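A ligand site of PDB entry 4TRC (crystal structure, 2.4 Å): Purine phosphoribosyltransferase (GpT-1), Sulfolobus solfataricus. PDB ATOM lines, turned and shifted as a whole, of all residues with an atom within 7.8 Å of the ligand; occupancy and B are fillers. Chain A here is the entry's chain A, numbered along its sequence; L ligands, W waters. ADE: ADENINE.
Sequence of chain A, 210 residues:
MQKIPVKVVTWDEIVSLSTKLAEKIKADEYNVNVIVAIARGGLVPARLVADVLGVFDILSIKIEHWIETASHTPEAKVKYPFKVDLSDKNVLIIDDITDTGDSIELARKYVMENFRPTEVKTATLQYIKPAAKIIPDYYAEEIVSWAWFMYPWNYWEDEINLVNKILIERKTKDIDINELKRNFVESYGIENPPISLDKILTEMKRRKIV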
ATOM      1  N   PRO A   5     -14.556 -28.415 -17.770  1.00  0.00           N
ATOM      2  CA  PRO A   5     -14.623 -26.956 -17.764  1.00  0.00           C
ATOM      3  C   PRO A   5     -14.500 -26.443 -19.199  1.00  0.00           C
ATOM      4  O   PRO A   5     -13.481 -26.663 -19.853  1.00  0.00           O
ATOM      5  CB  PRO A   5     -13.387 -26.537 -16.949  1.00  0.00           C
ATOM      6  CG  PRO A   5     -12.850 -27.798 -16.360  1.00  0.00           C
ATOM      7  CD  PRO A   5     -13.271 -28.902 -17.267  1.00  0.00           C
ATOM      8  N   LYS A   7     -14.911 -23.045 -21.779  1.00  0.00           N
ATOM      9  CA  LYS A   7     -15.123 -21.604 -21.939  1.00  0.00           C
ATOM     10  C   LYS A   7     -15.427 -21.212 -23.389  1.00  0.00           C
ATOM     11  O   LYS A   7     -14.620 -21.409 -24.294  1.00  0.00           O
ATOM     12  CB  LYS A   7     -13.942 -20.791 -21.400  1.00  0.00           C
ATOM     13  CG  LYS A   7     -14.086 -20.404 -19.919  1.00  0.00           C
ATOM     14  CD  LYS A   7     -13.416 -21.397 -18.971  1.00  0.00           C
ATOM     15  CE  LYS A   7     -14.018 -21.357 -17.572  1.00  0.00           C
ATOM     16  NZ  LYS A   7     -15.372 -21.992 -17.554  1.00  0.00           N
ATOM     17  N   GLY A  41      -5.090 -23.880 -35.742  1.00  0.00           N
ATOM     18  CA  GLY A  41      -5.512 -23.006 -34.648  1.00  0.00           C
ATOM     19  C   GLY A  41      -4.971 -21.587 -34.694  1.00  0.00           C
ATOM     20  O   GLY A  41      -5.560 -20.662 -34.155  1.00  0.00           O
ATOM     21  N   HIS A  65      -1.404 -34.129 -34.057  1.00  0.00           N
ATOM     22  CA  HIS A  65      -1.129 -34.690 -32.743  1.00  0.00           C
ATOM     23  C   HIS A  65      -1.537 -36.162 -32.680  1.00  0.00           C
ATOM     24  O   HIS A  65      -2.705 -36.512 -32.882  1.00  0.00           O
ATOM     25  CB  HIS A  65      -1.822 -33.852 -31.673  1.00  0.00           C
ATOM     26  CG  HIS A  65      -1.400 -32.417 -31.685  1.00  0.00           C
ATOM     27  ND1 HIS A  65      -2.027 -31.457 -32.460  1.00  0.00           N
ATOM     28  CD2 HIS A  65      -0.376 -31.784 -31.060  1.00  0.00           C
ATOM     29  CE1 HIS A  65      -1.424 -30.304 -32.293  1.00  0.00           C
ATOM     30  NE2 HIS A  65      -0.420 -30.470 -31.445  1.00  0.00           N
ATOM     31  N   ASP A  95       0.070 -19.278 -32.644  1.00  0.00           N
ATOM     32  CA  ASP A  95      -0.972 -20.280 -32.435  1.00  0.00           C
ATOM     33  C   ASP A  95      -2.048 -19.722 -31.501  1.00  0.00           C
ATOM     34  O   ASP A  95      -1.840 -18.692 -30.876  1.00  0.00           O
ATOM     35  CB  ASP A  95      -0.377 -21.551 -31.827  1.00  0.00           C
ATOM     36  CG  ASP A  95      -1.201 -22.794 -32.143  1.00  0.00           C
ATOM     37  OD1 ASP A  95      -2.230 -22.663 -32.853  1.00  0.00           O
ATOM     38  OD2 ASP A  95      -0.815 -23.910 -31.700  1.00  0.00           O
ATOM     39  N   ASP A  96      -3.176 -20.421 -31.398  1.00  0.00           N
ATOM     40  CA  ASP A  96      -4.264 -19.982 -30.520  1.00  0.00           C
ATOM     41  C   ASP A  96      -3.945 -20.109 -29.010  1.00  0.00           C
ATOM     42  O   ASP A  96      -4.096 -19.148 -28.256  1.00  0.00           O
ATOM     43  CB  ASP A  96      -5.572 -20.697 -30.876  1.00  0.00           C
ATOM     44  CG  ASP A  96      -5.420 -22.208 -30.984  1.00  0.00           C
ATOM     45  OD1 ASP A  96      -4.325 -22.756 -30.719  1.00  0.00           O
ATOM     46  OD2 ASP A  96      -6.404 -22.877 -31.365  1.00  0.00           O
ATOM     47  N   ILE A  97      -3.494 -21.281 -28.585  1.00  0.00           N
ATOM     48  CA  ILE A  97      -3.285 -21.513 -27.156  1.00  0.00           C
ATOM     49  C   ILE A  97      -2.018 -22.349 -26.892  1.00  0.00           C
ATOM     50  O   ILE A  97      -1.703 -23.278 -27.635  1.00  0.00           O
ATOM     51  CB  ILE A  97      -4.548 -22.182 -26.508  1.00  0.00           C
ATOM     52  CG1 ILE A  97      -4.426 -22.290 -24.993  1.00  0.00           C
ATOM     53  CG2 ILE A  97      -4.838 -23.543 -27.130  1.00  0.00           C
ATOM     54  CD1 ILE A  97      -5.773 -22.479 -24.304  1.00  0.00           C
ATOM     55  N   THR A  98      -1.265 -21.981 -25.870  1.00  0.00           N
ATOM     56  CA  THR A  98      -0.240 -22.882 -25.377  1.00  0.00           C
ATOM     57  C   THR A  98      -0.838 -23.722 -24.257  1.00  0.00           C
ATOM     58  O   THR A  98      -1.128 -23.198 -23.181  1.00  0.00           O
ATOM     59  CB  THR A  98       0.956 -22.121 -24.826  1.00  0.00           C
ATOM     60  OG1 THR A  98       1.479 -21.267 -25.842  1.00  0.00           O
ATOM     61  CG2 THR A  98       2.029 -23.102 -24.383  1.00  0.00           C
ATOM     62  N   ASP A  99      -1.052 -25.013 -24.503  1.00  0.00           N
ATOM     63  CA  ASP A  99      -1.573 -25.893 -23.455  1.00  0.00           C
ATOM     64  C   ASP A  99      -0.445 -26.688 -22.781  1.00  0.00           C
ATOM     65  O   ASP A  99       0.042 -26.308 -21.718  1.00  0.00           O
ATOM     66  CB  ASP A  99      -2.662 -26.814 -24.021  1.00  0.00           C
ATOM     67  CG  ASP A  99      -3.447 -27.533 -22.943  1.00  0.00           C
ATOM     68  OD1 ASP A  99      -4.556 -28.029 -23.243  1.00  0.00           O
ATOM     69  OD2 ASP A  99      -2.958 -27.605 -21.799  1.00  0.00           O
ATOM     70  N   THR A 100      -0.018 -27.773 -23.423  1.00  0.00           N
ATOM     71  CA  THR A 100       1.174 -28.509 -22.968  1.00  0.00           C
ATOM     72  C   THR A 100       2.427 -27.777 -23.434  1.00  0.00           C
ATOM     73  O   THR A 100       3.472 -27.863 -22.802  1.00  0.00           O
ATOM     74  CB  THR A 100       1.239 -29.931 -23.563  1.00  0.00           C
ATOM     75  OG1 THR A 100       1.417 -29.843 -24.985  1.00  0.00           O
ATOM     76  CG2 THR A 100      -0.045 -30.708 -23.248  1.00  0.00           C
ATOM     77  N   SER A 103       3.147 -28.133 -29.135  1.00  0.00           N
ATOM     78  CA  SER A 103       3.027 -27.581 -30.488  1.00  0.00           C
ATOM     79  C   SER A 103       4.036 -26.478 -30.787  1.00  0.00           C
ATOM     80  O   SER A 103       4.734 -26.529 -31.795  1.00  0.00           O
ATOM     81  CB  SER A 103       1.601 -27.094 -30.731  1.00  0.00           C
ATOM     82  OG  SER A 103       0.687 -28.162 -30.564  1.00  0.00           O
ATOM     83  N   GLN A 126      -3.670 -17.445 -25.712  1.00  0.00           N
ATOM     84  CA  GLN A 126      -3.759 -17.922 -24.329  1.00  0.00           C
ATOM     85  C   GLN A 126      -2.640 -18.859 -23.951  1.00  0.00           C
ATOM     86  O   GLN A 126      -2.038 -19.499 -24.799  1.00  0.00           O
ATOM     87  CB  GLN A 126      -5.119 -18.544 -24.080  1.00  0.00           C
ATOM     88  CG  GLN A 126      -6.163 -17.479 -23.770  1.00  0.00           C
ATOM     89  CD  GLN A 126      -7.524 -17.783 -24.314  1.00  0.00           C
ATOM     90  OE1 GLN A 126      -8.524 -17.200 -23.886  1.00  0.00           O
ATOM     91  NE2 GLN A 126      -7.581 -18.707 -25.259  1.00  0.00           N
ATOM     92  N   ILE A 128      -1.690 -21.567 -20.658  1.00  0.00           N
ATOM     93  CA  ILE A 128      -2.120 -22.244 -19.441  1.00  0.00           C
ATOM     94  C   ILE A 128      -0.936 -22.535 -18.545  1.00  0.00           C
ATOM     95  O   ILE A 128      -0.238 -23.530 -18.716  1.00  0.00           O
ATOM     96  CB  ILE A 128      -2.894 -23.533 -19.737  1.00  0.00           C
ATOM     97  CG1 ILE A 128      -3.925 -23.290 -20.837  1.00  0.00           C
ATOM     98  CG2 ILE A 128      -3.551 -24.047 -18.467  1.00  0.00           C
ATOM     99  CD1 ILE A 128      -4.914 -24.436 -21.005  1.00  0.00           C
ATOM    100  N   ALA A 131      -0.237 -26.062 -17.067  1.00  0.00           N
ATOM    101  CA  ALA A 131      -0.053 -27.149 -18.036  1.00  0.00           C
ATOM    102  C   ALA A 131       1.198 -27.029 -18.907  1.00  0.00           C
ATOM    103  O   ALA A 131       1.734 -28.039 -19.366  1.00  0.00           O
ATOM    104  CB  ALA A 131      -1.291 -27.301 -18.914  1.00  0.00           C
ATOM    105  N   ILE A 143      -3.850 -18.250 -18.272  1.00  0.00           N
ATOM    106  CA  ILE A 143      -4.897 -19.072 -17.695  1.00  0.00           C
ATOM    107  C   ILE A 143      -4.271 -19.895 -16.559  1.00  0.00           C
ATOM    108  O   ILE A 143      -3.253 -20.566 -16.751  1.00  0.00           O
ATOM    109  CB  ILE A 143      -5.479 -20.027 -18.740  1.00  0.00           C
ATOM    110  CG1 ILE A 143      -5.982 -19.224 -19.938  1.00  0.00           C
ATOM    111  CG2 ILE A 143      -6.596 -20.853 -18.141  1.00  0.00           C
ATOM    112  CD1 ILE A 143      -7.098 -18.217 -19.565  1.00  0.00           C
ATOM    113  N   TRP A 146      -6.861 -24.990 -15.859  1.00  0.00           N
ATOM    114  CA  TRP A 146      -7.186 -25.659 -17.131  1.00  0.00           C
ATOM    115  C   TRP A 146      -8.662 -25.621 -17.507  1.00  0.00           C
ATOM    116  O   TRP A 146      -9.541 -25.849 -16.666  1.00  0.00           O
ATOM    117  CB  TRP A 146      -6.745 -27.118 -17.141  1.00  0.00           C
ATOM    118  CG  TRP A 146      -6.708 -27.709 -18.519  1.00  0.00           C
ATOM    119  CD1 TRP A 146      -5.636 -27.748 -19.357  1.00  0.00           C
ATOM    120  CD2 TRP A 146      -7.806 -28.305 -19.237  1.00  0.00           C
ATOM    121  NE1 TRP A 146      -5.992 -28.347 -20.538  1.00  0.00           N
ATOM    122  CE2 TRP A 146      -7.322 -28.683 -20.492  1.00  0.00           C
ATOM    123  CE3 TRP A 146      -9.148 -28.535 -18.936  1.00  0.00           C
ATOM    124  CZ2 TRP A 146      -8.120 -29.319 -21.450  1.00  0.00           C
ATOM    125  CZ3 TRP A 146      -9.937 -29.158 -19.879  1.00  0.00           C
ATOM    126  CH2 TRP A 146      -9.436 -29.541 -21.120  1.00  0.00           C
ATOM    127  N   ALA A 147      -8.932 -25.347 -18.769  1.00  0.00           N
ATOM    128  CA  ALA A 147     -10.281 -25.410 -19.300  1.00  0.00           C
ATOM    129  C   ALA A 147     -10.149 -25.636 -20.782  1.00  0.00           C
ATOM    130  O   ALA A 147      -9.069 -25.459 -21.355  1.00  0.00           O
ATOM    131  CB  ALA A 147     -11.028 -24.122 -19.021  1.00  0.00           C
ATOM    132  N   TRP A 148     -11.228 -26.082 -21.404  1.00  0.00           N
ATOM    133  CA  TRP A 148     -11.222 -26.193 -22.858  1.00  0.00           C
ATOM    134  C   TRP A 148     -11.739 -24.891 -23.433  1.00  0.00           C
ATOM    135  O   TRP A 148     -12.861 -24.463 -23.159  1.00  0.00           O
ATOM    136  CB  TRP A 148     -12.059 -27.365 -23.355  1.00  0.00           C
ATOM    137  CG  TRP A 148     -11.940 -27.498 -24.821  1.00  0.00           C
ATOM    138  CD1 TRP A 148     -12.841 -27.087 -25.765  1.00  0.00           C
ATOM    139  CD2 TRP A 148     -10.831 -28.053 -25.554  1.00  0.00           C
ATOM    140  NE1 TRP A 148     -12.377 -27.370 -27.039  1.00  0.00           N
ATOM    141  CE2 TRP A 148     -11.139 -27.968 -26.927  1.00  0.00           C
ATOM    142  CE3 TRP A 148      -9.620 -28.634 -25.167  1.00  0.00           C
ATOM    143  CZ2 TRP A 148     -10.283 -28.429 -27.921  1.00  0.00           C
ATOM    144  CZ3 TRP A 148      -8.770 -29.099 -26.154  1.00  0.00           C
ATOM    145  CH2 TRP A 148      -9.091 -28.990 -27.508  1.00  0.00           C
ATOM    146  N   PHE A 149     -10.920 -24.236 -24.243  1.00  0.00           N
ATOM    147  CA  PHE A 149     -11.349 -22.986 -24.856  1.00  0.00           C
ATOM    148  C   PHE A 149     -11.976 -23.225 -26.209  1.00  0.00           C
ATOM    149  O   PHE A 149     -11.373 -23.775 -27.121  1.00  0.00           O
ATOM    150  CB  PHE A 149     -10.218 -21.980 -24.915  1.00  0.00           C
ATOM    151  CG  PHE A 149      -9.816 -21.490 -23.560  1.00  0.00           C
ATOM    152  CD1 PHE A 149      -8.911 -22.206 -22.790  1.00  0.00           C
ATOM    153  CD2 PHE A 149     -10.408 -20.352 -23.028  1.00  0.00           C
ATOM    154  CE1 PHE A 149      -8.563 -21.772 -21.522  1.00  0.00           C
ATOM    155  CE2 PHE A 149     -10.067 -19.922 -21.754  1.00  0.00           C
ATOM    156  CZ  PHE A 149      -9.149 -20.629 -20.997  1.00  0.00           C
ATOM    157  N   MET A 150     -13.231 -22.829 -26.297  1.00  0.00           N
ATOM    158  CA  MET A 150     -14.008 -23.018 -27.503  1.00  0.00           C
ATOM    159  C   MET A 150     -13.926 -21.742 -28.356  1.00  0.00           C
ATOM    160  O   MET A 150     -14.621 -20.750 -28.092  1.00  0.00           O
ATOM    161  CB  MET A 150     -15.438 -23.309 -27.096  1.00  0.00           C
ATOM    162  CG  MET A 150     -16.235 -24.092 -28.102  1.00  0.00           C
ATOM    163  SD  MET A 150     -17.789 -24.669 -27.355  1.00  0.00           S
ATOM    164  CE  MET A 150     -18.828 -24.269 -28.730  1.00  0.00           C
ATOM    165  N   TYR A 151     -13.072 -21.774 -29.369  1.00  0.00           N
ATOM    166  CA  TYR A 151     -12.881 -20.612 -30.235  1.00  0.00           C
ATOM    167  C   TYR A 151     -13.961 -20.520 -31.310  1.00  0.00           C
ATOM    168  O   TYR A 151     -14.512 -21.550 -31.715  1.00  0.00           O
ATOM    169  CB  TYR A 151     -11.485 -20.620 -30.879  1.00  0.00           C
ATOM    170  CG  TYR A 151     -10.390 -20.621 -29.839  1.00  0.00           C
ATOM    171  CD1 TYR A 151      -9.543 -21.712 -29.699  1.00  0.00           C
ATOM    172  CD2 TYR A 151     -10.215 -19.537 -28.968  1.00  0.00           C
ATOM    173  CE1 TYR A 151      -8.547 -21.722 -28.745  1.00  0.00           C
ATOM    174  CE2 TYR A 151      -9.226 -19.551 -28.007  1.00  0.00           C
ATOM    175  CZ  TYR A 151      -8.398 -20.646 -27.903  1.00  0.00           C
ATOM    176  OH  TYR A 151      -7.411 -20.670 -26.952  1.00  0.00           O
ATOM    177  N   TRP A 153     -13.875 -20.091 -34.330  1.00  0.00           N
ATOM    178  CA  TRP A 153     -13.564 -20.787 -35.586  1.00  0.00           C
ATOM    179  C   TRP A 153     -13.591 -22.294 -35.376  1.00  0.00           C
ATOM    180  O   TRP A 153     -13.168 -23.050 -36.242  1.00  0.00           O
ATOM    181  CB  TRP A 153     -12.210 -20.364 -36.120  1.00  0.00           C
ATOM    182  CG  TRP A 153     -11.116 -20.556 -35.141  1.00  0.00           C
ATOM    183  CD1 TRP A 153     -10.527 -21.727 -34.796  1.00  0.00           C
ATOM    184  CD2 TRP A 153     -10.495 -19.550 -34.347  1.00  0.00           C
ATOM    185  NE1 TRP A 153      -9.557 -21.513 -33.847  1.00  0.00           N
ATOM    186  CE2 TRP A 153      -9.521 -20.182 -33.549  1.00  0.00           C
ATOM    187  CE3 TRP A 153     -10.668 -18.162 -34.230  1.00  0.00           C
ATOM    188  CZ2 TRP A 153      -8.726 -19.480 -32.657  1.00  0.00           C
ATOM    189  CZ3 TRP A 153      -9.875 -17.474 -33.334  1.00  0.00           C
ATOM    190  CH2 TRP A 153      -8.902 -18.133 -32.569  1.00  0.00           C
ATOM    191  N   ASN A 154     -14.105 -22.730 -34.224  1.00  0.00           N
ATOM    192  CA  ASN A 154     -14.059 -24.133 -33.833  1.00  0.00           C
ATOM    193  C   ASN A 154     -15.411 -24.610 -33.301  1.00  0.00           C
ATOM    194  O   ASN A 154     -15.527 -25.728 -32.809  1.00  0.00           O
ATOM    195  CB  ASN A 154     -12.996 -24.292 -32.740  1.00  0.00           C
ATOM    196  CG  ASN A 154     -12.006 -25.393 -33.048  1.00  0.00           C
ATOM    197  OD1 ASN A 154     -10.804 -25.183 -32.978  1.00  0.00           O
ATOM    198  ND2 ASN A 154     -12.504 -26.582 -33.366  1.00  0.00           N
ATOM    199  N   ASP A 158     -15.916 -28.482 -32.089  1.00  0.00           N
ATOM    200  CA  ASP A 158     -15.916 -28.604 -30.639  1.00  0.00           C
ATOM    201  C   ASP A 158     -17.260 -29.129 -30.130  1.00  0.00           C
ATOM    202  O   ASP A 158     -17.320 -29.983 -29.263  1.00  0.00           O
ATOM    203  CB  ASP A 158     -15.622 -27.254 -30.004  1.00  0.00           C
ATOM    204  CG  ASP A 158     -14.145 -26.992 -29.864  1.00  0.00           C
ATOM    205  OD1 ASP A 158     -13.341 -27.863 -30.267  1.00  0.00           O
ATOM    206  OD2 ASP A 158     -13.800 -25.923 -29.342  1.00  0.00           O
HETATM  207  N9  ADE L   1      -6.021 -27.142 -28.080  1.00  0.00           N
HETATM  208  C8  ADE L   1      -5.119 -27.772 -27.166  1.00  0.00           C
HETATM  209  N7  ADE L   1      -5.518 -27.474 -25.926  1.00  0.00           N
HETATM  210  C5  ADE L   1      -6.627 -26.683 -26.021  1.00  0.00           C
HETATM  211  C6  ADE L   1      -7.438 -26.097 -25.043  1.00  0.00           C
HETATM  212  N6  ADE L   1      -7.135 -26.274 -23.671  1.00  0.00           N
HETATM  213  N1  ADE L   1      -8.508 -25.350 -25.418  1.00  0.00           N
HETATM  214  C2  ADE L   1      -8.790 -25.165 -26.717  1.00  0.00           C
HETATM  215  N3  ADE L   1      -7.955 -25.777 -27.736  1.00  0.00           N
HETATM  216  C4  ADE L   1      -6.922 -26.494 -27.376  1.00  0.00           C
HETATM  217  O   HOH W   1      -9.355 -25.656 -30.215  1.00  0.00           O
HETATM  218  O   HOH W   2      -2.950 -28.924 -29.607  1.00  0.00           O
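Water W1 bridges N3 of the ligand (2.8 Å) and OD1 of Asn 154 (3.2 Å).
The backbone carbonyl oxygen of Ala 147 lies within hydrogen-bond range of a nitrogen (N6) of the ligand. The side-chain carboxylate (OD1) of Asp 99 lies within hydrogen-bond range of a nitrogen (N6) of the ligand (3.1 Å). N of Phe 149 sits at hydrogen-bond distance from N1 of the ligand (2.9 Å).
OD1 of Asp 99 sits at hydrogen-bond distance from NE1 of Trp 146 (3.1 Å). The backbone NH (N) of Ile 128 sits at hydrogen-bond distance from the backbone carbonyl oxygen (O) of Thr 98 (3.1 Å). The backbone NH (N) of Trp 148 sits at hydrogen-bond distance from the backbone carbonyl oxygen (O) of Pro 5, 2.8 Å away. The indole nitrogen of Trp 148 sits at hydrogen-bond distance from the side-chain carboxylate of Asp 158 (3.1 Å). The backbone carbonyl oxygen (O) of Trp 148 is in hydrogen-bond range of the backbone NH (N) of Lys 7 (2.8 Å).
Merely in contact with the ligand: Trp 148 (3.2 Å), Ile 97 (3.6 Å), Trp 146 (3.9 Å) and Ile 128 (3.9 Å). Seven residues have an atom within 4 Å of the ligand: Ile 97, Asp 99, Ile 128, Trp 146, Ala 147, Trp 148 and Phe 149. Along chain A the residues within 4 Å of the ligand span positions 97 to 149.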
